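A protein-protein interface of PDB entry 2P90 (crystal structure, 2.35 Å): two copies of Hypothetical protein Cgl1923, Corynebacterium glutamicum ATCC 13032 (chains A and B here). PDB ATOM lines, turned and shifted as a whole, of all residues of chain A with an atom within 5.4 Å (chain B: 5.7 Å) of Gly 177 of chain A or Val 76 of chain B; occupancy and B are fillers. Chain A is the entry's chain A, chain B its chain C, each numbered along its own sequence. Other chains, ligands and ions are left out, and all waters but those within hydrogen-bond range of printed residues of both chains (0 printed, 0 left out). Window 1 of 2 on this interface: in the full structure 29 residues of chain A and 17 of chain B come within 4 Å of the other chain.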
ATOM      1  N   TYR A  35       9.336 -24.172  23.248  1.00  0.00           N
ATOM      2  CA  TYR A  35       8.628 -23.350  22.252  1.00  0.00           C
ATOM      3  C   TYR A  35       9.475 -23.097  21.020  1.00  0.00           C
ATOM      4  O   TYR A  35       9.072 -23.483  19.938  1.00  0.00           O
ATOM      5  CB  TYR A  35       8.212 -21.987  22.833  1.00  0.00           C
ATOM      6  CG  TYR A  35       7.593 -21.022  21.793  1.00  0.00           C
ATOM      7  CD1 TYR A  35       6.412 -21.373  21.059  1.00  0.00           C
ATOM      8  CD2 TYR A  35       8.160 -19.755  21.575  1.00  0.00           C
ATOM      9  CE1 TYR A  35       5.863 -20.505  20.144  1.00  0.00           C
ATOM     10  CE2 TYR A  35       7.634 -18.865  20.660  1.00  0.00           C
ATOM     11  CZ  TYR A  35       6.469 -19.239  19.947  1.00  0.00           C
ATOM     12  OH  TYR A  35       5.916 -18.326  19.076  1.00  0.00           O
ATOM     13  N   GLU A 111       9.228 -24.461  29.552  1.00  0.00           N
ATOM     14  CA  GLU A 111       8.046 -23.649  29.327  1.00  0.00           C
ATOM     15  C   GLU A 111       6.833 -24.365  29.932  1.00  0.00           C
ATOM     16  O   GLU A 111       6.593 -25.496  29.640  1.00  0.00           O
ATOM     17  CB  GLU A 111       7.793 -23.408  27.851  1.00  0.00           C
ATOM     18  CG  GLU A 111       6.381 -22.839  27.549  1.00  0.00           C
ATOM     19  CD  GLU A 111       6.063 -22.813  26.056  1.00  0.00           C
ATOM     20  OE1 GLU A 111       6.308 -23.825  25.344  1.00  0.00           O
ATOM     21  OE2 GLU A 111       5.520 -21.780  25.590  1.00  0.00           O
ATOM     22  N   TRP A 116      -0.847 -20.423  32.159  1.00  0.00           N
ATOM     23  CA  TRP A 116      -0.070 -19.307  31.625  1.00  0.00           C
ATOM     24  C   TRP A 116      -0.411 -17.979  32.276  1.00  0.00           C
ATOM     25  O   TRP A 116       0.479 -17.180  32.475  1.00  0.00           O
ATOM     26  CB  TRP A 116      -0.196 -19.223  30.097  1.00  0.00           C
ATOM     27  CG  TRP A 116       0.630 -20.244  29.354  1.00  0.00           C
ATOM     28  CD1 TRP A 116       1.284 -21.359  29.891  1.00  0.00           C
ATOM     29  CD2 TRP A 116       0.827 -20.316  27.938  1.00  0.00           C
ATOM     30  NE1 TRP A 116       1.873 -22.082  28.885  1.00  0.00           N
ATOM     31  CE2 TRP A 116       1.611 -21.480  27.684  1.00  0.00           C
ATOM     32  CE3 TRP A 116       0.401 -19.517  26.845  1.00  0.00           C
ATOM     33  CZ2 TRP A 116       2.000 -21.844  26.401  1.00  0.00           C
ATOM     34  CZ3 TRP A 116       0.779 -19.871  25.582  1.00  0.00           C
ATOM     35  CH2 TRP A 116       1.572 -21.028  25.363  1.00  0.00           C
ATOM     36  N   MET A 173       3.548  -9.730  12.014  1.00  0.00           N
ATOM     37  CA  MET A 173       3.483 -11.189  11.950  1.00  0.00           C
ATOM     38  C   MET A 173       2.635 -11.863  13.049  1.00  0.00           C
ATOM     39  O   MET A 173       2.379 -11.297  14.130  1.00  0.00           O
ATOM     40  CB  MET A 173       4.894 -11.810  11.853  1.00  0.00           C
ATOM     41  CG  MET A 173       5.852 -11.361  12.948  1.00  0.00           C
ATOM     42  SD  MET A 173       7.566 -11.881  12.680  1.00  0.00           S
ATOM     43  CE  MET A 173       8.400 -10.457  13.392  1.00  0.00           C
ATOM     44  N   THR A 174       2.203 -13.075  12.726  1.00  0.00           N
ATOM     45  CA  THR A 174       1.313 -13.871  13.547  1.00  0.00           C
ATOM     46  C   THR A 174       2.083 -15.133  13.870  1.00  0.00           C
ATOM     47  O   THR A 174       2.522 -15.813  12.947  1.00  0.00           O
ATOM     48  CB  THR A 174       0.040 -14.234  12.742  1.00  0.00           C
ATOM     49  OG1 THR A 174      -0.706 -13.039  12.470  1.00  0.00           O
ATOM     50  CG2 THR A 174      -0.835 -15.186  13.498  1.00  0.00           C
ATOM     51  N   VAL A 175       2.294 -15.422  15.156  1.00  0.00           N
ATOM     52  CA  VAL A 175       3.024 -16.641  15.572  1.00  0.00           C
ATOM     53  C   VAL A 175       2.200 -17.451  16.578  1.00  0.00           C
ATOM     54  O   VAL A 175       1.378 -16.872  17.284  1.00  0.00           O
ATOM     55  CB  VAL A 175       4.411 -16.314  16.189  1.00  0.00           C
ATOM     56  CG1 VAL A 175       5.359 -15.706  15.126  1.00  0.00           C
ATOM     57  CG2 VAL A 175       4.282 -15.390  17.446  1.00  0.00           C
ATOM     58  N   PRO A 176       2.431 -18.781  16.677  1.00  0.00           N
ATOM     59  CA  PRO A 176       1.733 -19.430  17.795  1.00  0.00           C
ATOM     60  C   PRO A 176       2.213 -18.841  19.131  1.00  0.00           C
ATOM     61  O   PRO A 176       3.390 -18.419  19.278  1.00  0.00           O
ATOM     62  CB  PRO A 176       2.110 -20.917  17.657  1.00  0.00           C
ATOM     63  CG  PRO A 176       2.591 -21.087  16.228  1.00  0.00           C
ATOM     64  CD  PRO A 176       3.270 -19.741  15.922  1.00  0.00           C
ATOM     65  N   GLY A 177       1.299 -18.771  20.085  1.00  0.00           N
ATOM     66  CA  GLY A 177       1.602 -18.162  21.375  1.00  0.00           C
ATOM     67  C   GLY A 177       2.480 -19.020  22.267  1.00  0.00           C
ATOM     68  O   GLY A 177       2.583 -20.231  22.071  1.00  0.00           O
ATOM     69  N   SER A 178       3.151 -18.364  23.221  1.00  0.00           N
ATOM     70  CA  SER A 178       3.985 -19.045  24.181  1.00  0.00           C
ATOM     71  C   SER A 178       3.796 -18.393  25.529  1.00  0.00           C
ATOM     72  O   SER A 178       3.286 -17.279  25.589  1.00  0.00           O
ATOM     73  CB  SER A 178       5.445 -19.026  23.732  1.00  0.00           C
ATOM     74  OG  SER A 178       6.068 -17.785  23.969  1.00  0.00           O
ATOM     75  N   ALA A 179       4.188 -19.086  26.607  1.00  0.00           N
ATOM     76  CA  ALA A 179       4.202 -18.504  27.945  1.00  0.00           C
ATOM     77  C   ALA A 179       5.048 -17.215  28.052  1.00  0.00           C
ATOM     78  O   ALA A 179       4.633 -16.256  28.715  1.00  0.00           O
ATOM     79  CB  ALA A 179       4.664 -19.557  28.957  1.00  0.00           C
ATOM     80  N   LEU A 181       5.641 -15.135  25.558  1.00  0.00           N
ATOM     81  CA  LEU A 181       4.944 -14.102  24.798  1.00  0.00           C
ATOM     82  C   LEU A 181       3.806 -13.466  25.607  1.00  0.00           C
ATOM     83  O   LEU A 181       3.623 -12.228  25.578  1.00  0.00           O
ATOM     84  CB  LEU A 181       4.477 -14.638  23.443  1.00  0.00           C
ATOM     85  CG  LEU A 181       5.636 -14.889  22.432  1.00  0.00           C
ATOM     86  CD1 LEU A 181       5.171 -15.648  21.173  1.00  0.00           C
ATOM     87  CD2 LEU A 181       6.278 -13.595  21.993  1.00  0.00           C
ATOM     88  N   TYR B  69      -2.161 -24.914  27.366  1.00  0.00           N
ATOM     89  CA  TYR B  69      -1.805 -23.856  26.472  1.00  0.00           C
ATOM     90  C   TYR B  69      -0.734 -24.271  25.479  1.00  0.00           C
ATOM     91  O   TYR B  69      -0.759 -23.785  24.365  1.00  0.00           O
ATOM     92  CB  TYR B  69      -1.315 -22.662  27.255  1.00  0.00           C
ATOM     93  CG  TYR B  69      -2.311 -21.916  28.085  1.00  0.00           C
ATOM     94  CD1 TYR B  69      -2.942 -20.791  27.577  1.00  0.00           C
ATOM     95  CD2 TYR B  69      -2.583 -22.303  29.407  1.00  0.00           C
ATOM     96  CE1 TYR B  69      -3.864 -20.057  28.348  1.00  0.00           C
ATOM     97  CE2 TYR B  69      -3.510 -21.588  30.194  1.00  0.00           C
ATOM     98  CZ  TYR B  69      -4.132 -20.474  29.664  1.00  0.00           C
ATOM     99  OH  TYR B  69      -5.009 -19.745  30.422  1.00  0.00           O
ATOM    100  N   ARG B  73      -1.590 -22.946  22.003  1.00  0.00           N
ATOM    101  CA  ARG B  73      -0.735 -21.832  21.557  1.00  0.00           C
ATOM    102  C   ARG B  73      -1.597 -20.666  20.956  1.00  0.00           C
ATOM    103  O   ARG B  73      -1.588 -20.402  19.739  1.00  0.00           O
ATOM    104  CB  ARG B  73       0.454 -22.321  20.665  1.00  0.00           C
ATOM    105  CG  ARG B  73       1.123 -23.627  21.185  1.00  0.00           C
ATOM    106  CD  ARG B  73       2.632 -23.890  20.844  1.00  0.00           C
ATOM    107  NE  ARG B  73       3.323 -23.076  21.791  1.00  0.00           N
ATOM    108  CZ  ARG B  73       4.241 -23.403  22.688  1.00  0.00           C
ATOM    109  NH1 ARG B  73       4.823 -24.590  22.792  1.00  0.00           N
ATOM    110  NH2 ARG B  73       4.626 -22.397  23.454  1.00  0.00           N
ATOM    111  N   PRO B  74      -2.400 -20.016  21.823  1.00  0.00           N
ATOM    112  CA  PRO B  74      -3.222 -18.922  21.317  1.00  0.00           C
ATOM    113  C   PRO B  74      -2.352 -17.912  20.547  1.00  0.00           C
ATOM    114  O   PRO B  74      -1.309 -17.459  21.036  1.00  0.00           O
ATOM    115  CB  PRO B  74      -3.809 -18.296  22.579  1.00  0.00           C
ATOM    116  CG  PRO B  74      -3.712 -19.327  23.635  1.00  0.00           C
ATOM    117  CD  PRO B  74      -2.573 -20.243  23.274  1.00  0.00           C
ATOM    118  N   VAL B  75      -2.825 -17.562  19.355  1.00  0.00           N
ATOM    119  CA  VAL B  75      -2.052 -16.866  18.361  1.00  0.00           C
ATOM    120  C   VAL B  75      -1.639 -15.459  18.821  1.00  0.00           C
ATOM    121  O   VAL B  75      -2.412 -14.738  19.433  1.00  0.00           O
ATOM    122  CB  VAL B  75      -2.843 -16.855  17.026  1.00  0.00           C
ATOM    123  CG1 VAL B  75      -2.389 -15.747  16.156  1.00  0.00           C
ATOM    124  CG2 VAL B  75      -2.651 -18.210  16.322  1.00  0.00           C
ATOM    125  N   VAL B  76      -0.398 -15.099  18.546  1.00  0.00           N
ATOM    126  CA  VAL B  76       0.132 -13.810  18.969  1.00  0.00           C
ATOM    127  C   VAL B  76       0.401 -12.937  17.735  1.00  0.00           C
ATOM    128  O   VAL B  76       0.892 -13.419  16.708  1.00  0.00           O
ATOM    129  CB  VAL B  76       1.403 -14.029  19.884  1.00  0.00           C
ATOM    130  CG1 VAL B  76       2.238 -12.778  20.050  1.00  0.00           C
ATOM    131  CG2 VAL B  76       0.974 -14.550  21.235  1.00  0.00           C
ATOM    132  N   VAL B  77       0.039 -11.659  17.821  1.00  0.00           N
ATOM    133  CA  VAL B  77       0.372 -10.710  16.761  1.00  0.00           C
ATOM    134  C   VAL B  77       1.502  -9.805  17.216  1.00  0.00           C
ATOM    135  O   VAL B  77       1.441  -9.208  18.288  1.00  0.00           O
ATOM    136  CB  VAL B  77      -0.883  -9.875  16.251  1.00  0.00           C
ATOM    137  CG1 VAL B  77      -0.457  -8.783  15.256  1.00  0.00           C
ATOM    138  CG2 VAL B  77      -1.918 -10.785  15.597  1.00  0.00           C
ATOM    139  N   ILE B  78       2.556  -9.754  16.411  1.00  0.00           N
ATOM    140  CA  ILE B  78       3.635  -8.782  16.596  1.00  0.00           C
ATOM    141  C   ILE B  78       3.570  -7.771  15.454  1.00  0.00           C
ATOM    142  O   ILE B  78       3.591  -8.142  14.277  1.00  0.00           O
ATOM    143  CB  ILE B  78       5.054  -9.466  16.714  1.00  0.00           C
ATOM    144  CG1 ILE B  78       5.110 -10.364  17.951  1.00  0.00           C
ATOM    145  CG2 ILE B  78       6.200  -8.414  16.804  1.00  0.00           C
ATOM    146  CD1 ILE B  78       5.974 -11.538  17.779  1.00  0.00           C
ATOM    147  N   VAL B  83       4.668  -7.035  20.781  1.00  0.00           N
ATOM    148  CA  VAL B  83       3.519  -7.904  20.899  1.00  0.00           C
ATOM    149  C   VAL B  83       2.321  -6.982  20.991  1.00  0.00           C
ATOM    150  O   VAL B  83       2.200  -6.207  21.937  1.00  0.00           O
ATOM    151  CB  VAL B  83       3.581  -8.797  22.161  1.00  0.00           C
ATOM    152  CG1 VAL B  83       2.373  -9.694  22.216  1.00  0.00           C
ATOM    153  CG2 VAL B  83       4.858  -9.625  22.183  1.00  0.00           C
ATOM    154  N   SER B  85      -0.971  -8.189  20.464  1.00  0.00           N
ATOM    155  CA  SER B  85      -2.209  -8.952  20.570  1.00  0.00           C
ATOM    156  C   SER B  85      -1.945 -10.399  20.859  1.00  0.00           C
ATOM    157  O   SER B  85      -1.057 -10.988  20.250  1.00  0.00           O
ATOM    158  CB  SER B  85      -2.926  -8.910  19.224  1.00  0.00           C
ATOM    159  OG  SER B  85      -4.266  -9.034  19.495  1.00  0.00           O
ATOM    160  N   MET B  86      -2.738 -10.971  21.765  1.00  0.00           N
ATOM    161  CA  MET B  86      -2.778 -12.418  22.006  1.00  0.00           C
ATOM    162  C   MET B  86      -4.239 -12.872  22.064  1.00  0.00           C
ATOM    163  O   MET B  86      -5.049 -12.326  22.824  1.00  0.00           O
ATOM    164  CB  MET B  86      -2.068 -12.768  23.316  1.00  0.00           C
ATOM    165  CG  MET B  86      -2.011 -14.310  23.637  1.00  0.00           C
ATOM    166  SD  MET B  86      -0.635 -14.691  24.767  1.00  0.00           S
ATOM    167  CE  MET B  86      -0.379 -16.438  24.551  1.00  0.00           C
ATOM    168  N   ASP B  87      -4.552 -13.899  21.300  1.00  0.00           N
ATOM    169  CA  ASP B  87      -5.873 -14.485  21.290  1.00  0.00           C
ATOM    170  C   ASP B  87      -6.257 -14.922  22.705  1.00  0.00           C
ATOM    171  O   ASP B  87      -5.560 -15.731  23.328  1.00  0.00           O
ATOM    172  CB  ASP B  87      -5.876 -15.679  20.347  1.00  0.00           C
ATOM    173  CG  ASP B  87      -7.279 -16.303  20.162  1.00  0.00           C
ATOM    174  OD1 ASP B  87      -8.265 -16.001  20.924  1.00  0.00           O
ATOM    175  OD2 ASP B  87      -7.371 -17.146  19.246  1.00  0.00           O
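NH2 of Arg 73 of chain B touches CD1 of Tyr 35 of chain A, at 3.2 Å.
Arg 73 of chain B touches Trp 116 of chain A (NH2 to CH2, 3.9 Å).
Trp 116 of chain A touches Met 86 of chain B.
Met 173 of chain A touches Val 76 of chain B (O to O, 3.7 Å).
O of Met 173 of chain A touches CA of Val 77 of chain B, 3.4 Å away.
Thr 174 of chain A touches Val 75 of chain B (CG2 to CG1, 3.1 Å).
Val 75 of chain B touches Val 175 of chain A (CA to O, 3.6 Å).
CB of Arg 73 of chain B touches CB of Pro 176 of chain A, at 3.7 Å.
Gly 177 of chain A touches Val 76 of chain B.
Arg 73 of chain B touches Ser 178 of chain A (NH2 to CB, 3.5 Å).
Printed residues of chain B that touch a printed residue of chain A: Tyr 69, Arg 73, Pro 74, Val 75, Val 76, Val 77, Ile 78 and Met 86.
Of the 11 printed residues of chain A, 9 touch a printed residue of chain B.
Hydrophobic or aromatic side chains of chain A that line the printed part of chain B: Tyr 35, Trp 116, Val 175 and Pro 176.
Along chain A the printed residues that touch a printed residue of chain B span positions 35 to 178.
Among the printed residues, Asp or Glu carboxylates within 4 Å of a Lys or Arg side-chain nitrogen of the other chain: Glu 111 of chain A with Arg 73 of chain B (2.4 Å).
O of Pro 176 of chain A sits at hydrogen-bond distance from OH of Tyr 35 of chain A (2.5 Å).
OE2 of Glu 111 of chain A is in hydrogen-bond range of N of Ala 179 of chain A, 3.2 Å away.
The side-chain hydroxyl of Ser 178 of chain A lies within hydrogen-bond range of the backbone NH of Leu 181 of chain A, at 3.1 Å.
The backbone carbonyl oxygen (O) of Val 75 of chain B lies within hydrogen-bond range of the backbone NH (N) of Asp 87 of chain B (3.0 Å).
The backbone NH of Val 77 of chain B lies within hydrogen-bond range of the backbone carbonyl oxygen of Ser 85 of chain B, 2.7 Å away.
No position is printed for both chains.
The side-chain carboxylate (OE1) of Glu 111 of chain A is in salt-bridge range of the guanidinium group (NH2) of Arg 73 of chain B (2.9 Å).
The backbone carbonyl oxygen (O) of Met 173 of chain A sits at hydrogen-bond distance from the backbone NH (N) of Ile 78 of chain B.
The backbone carbonyl oxygen of Val 175 of chain A sits at hydrogen-bond distance from the backbone NH of Val 76 of chain B (2.8 Å).
The backbone carbonyl oxygen (O) of Gly 177 of chain A lies within hydrogen-bond range of the guanidinium group (NE) of Arg 73 of chain B (3.0 Å).
The backbone NH (N) of Gly 177 of chain A lies close to the backbone carbonyl oxygen (O) of Pro 74 of chain B (3.1 Å).
Gly 177 of chain A touches just these residues of chain B: Arg 73, Pro 74 and Val 76.
Val 76 of chain B touches just these residues of chain A: Met 173, Thr 174, Val 175 and Gly 177.
Printed residues of chain A within 4 Å of Ile 78 of chain B: Met 173 (2.8 Å).
Of the printed residues of chain B, Pro 176 of chain A touches Arg 73 (3.7 Å).
Of the printed residues of chain B, Met 173 of chain A touches Val 76, Val 77 and Ile 78.
Of the printed residues of chain B, Glu 111 of chain A touches Arg 73.
Leu 181 of chain A touches none of the printed residues of chain B.
The nearest residue of chain B that does not touch Gly 177 of chain A is Met 86 of chain B (4.1 Å).
The nearest residue of chain A that does not touch Val 76 of chain B is Leu 181 of chain A (4.1 Å).
The nearest printed residue of chain A that does not touch Arg 73 of chain B is Ala 179 of chain A (4.6 Å).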
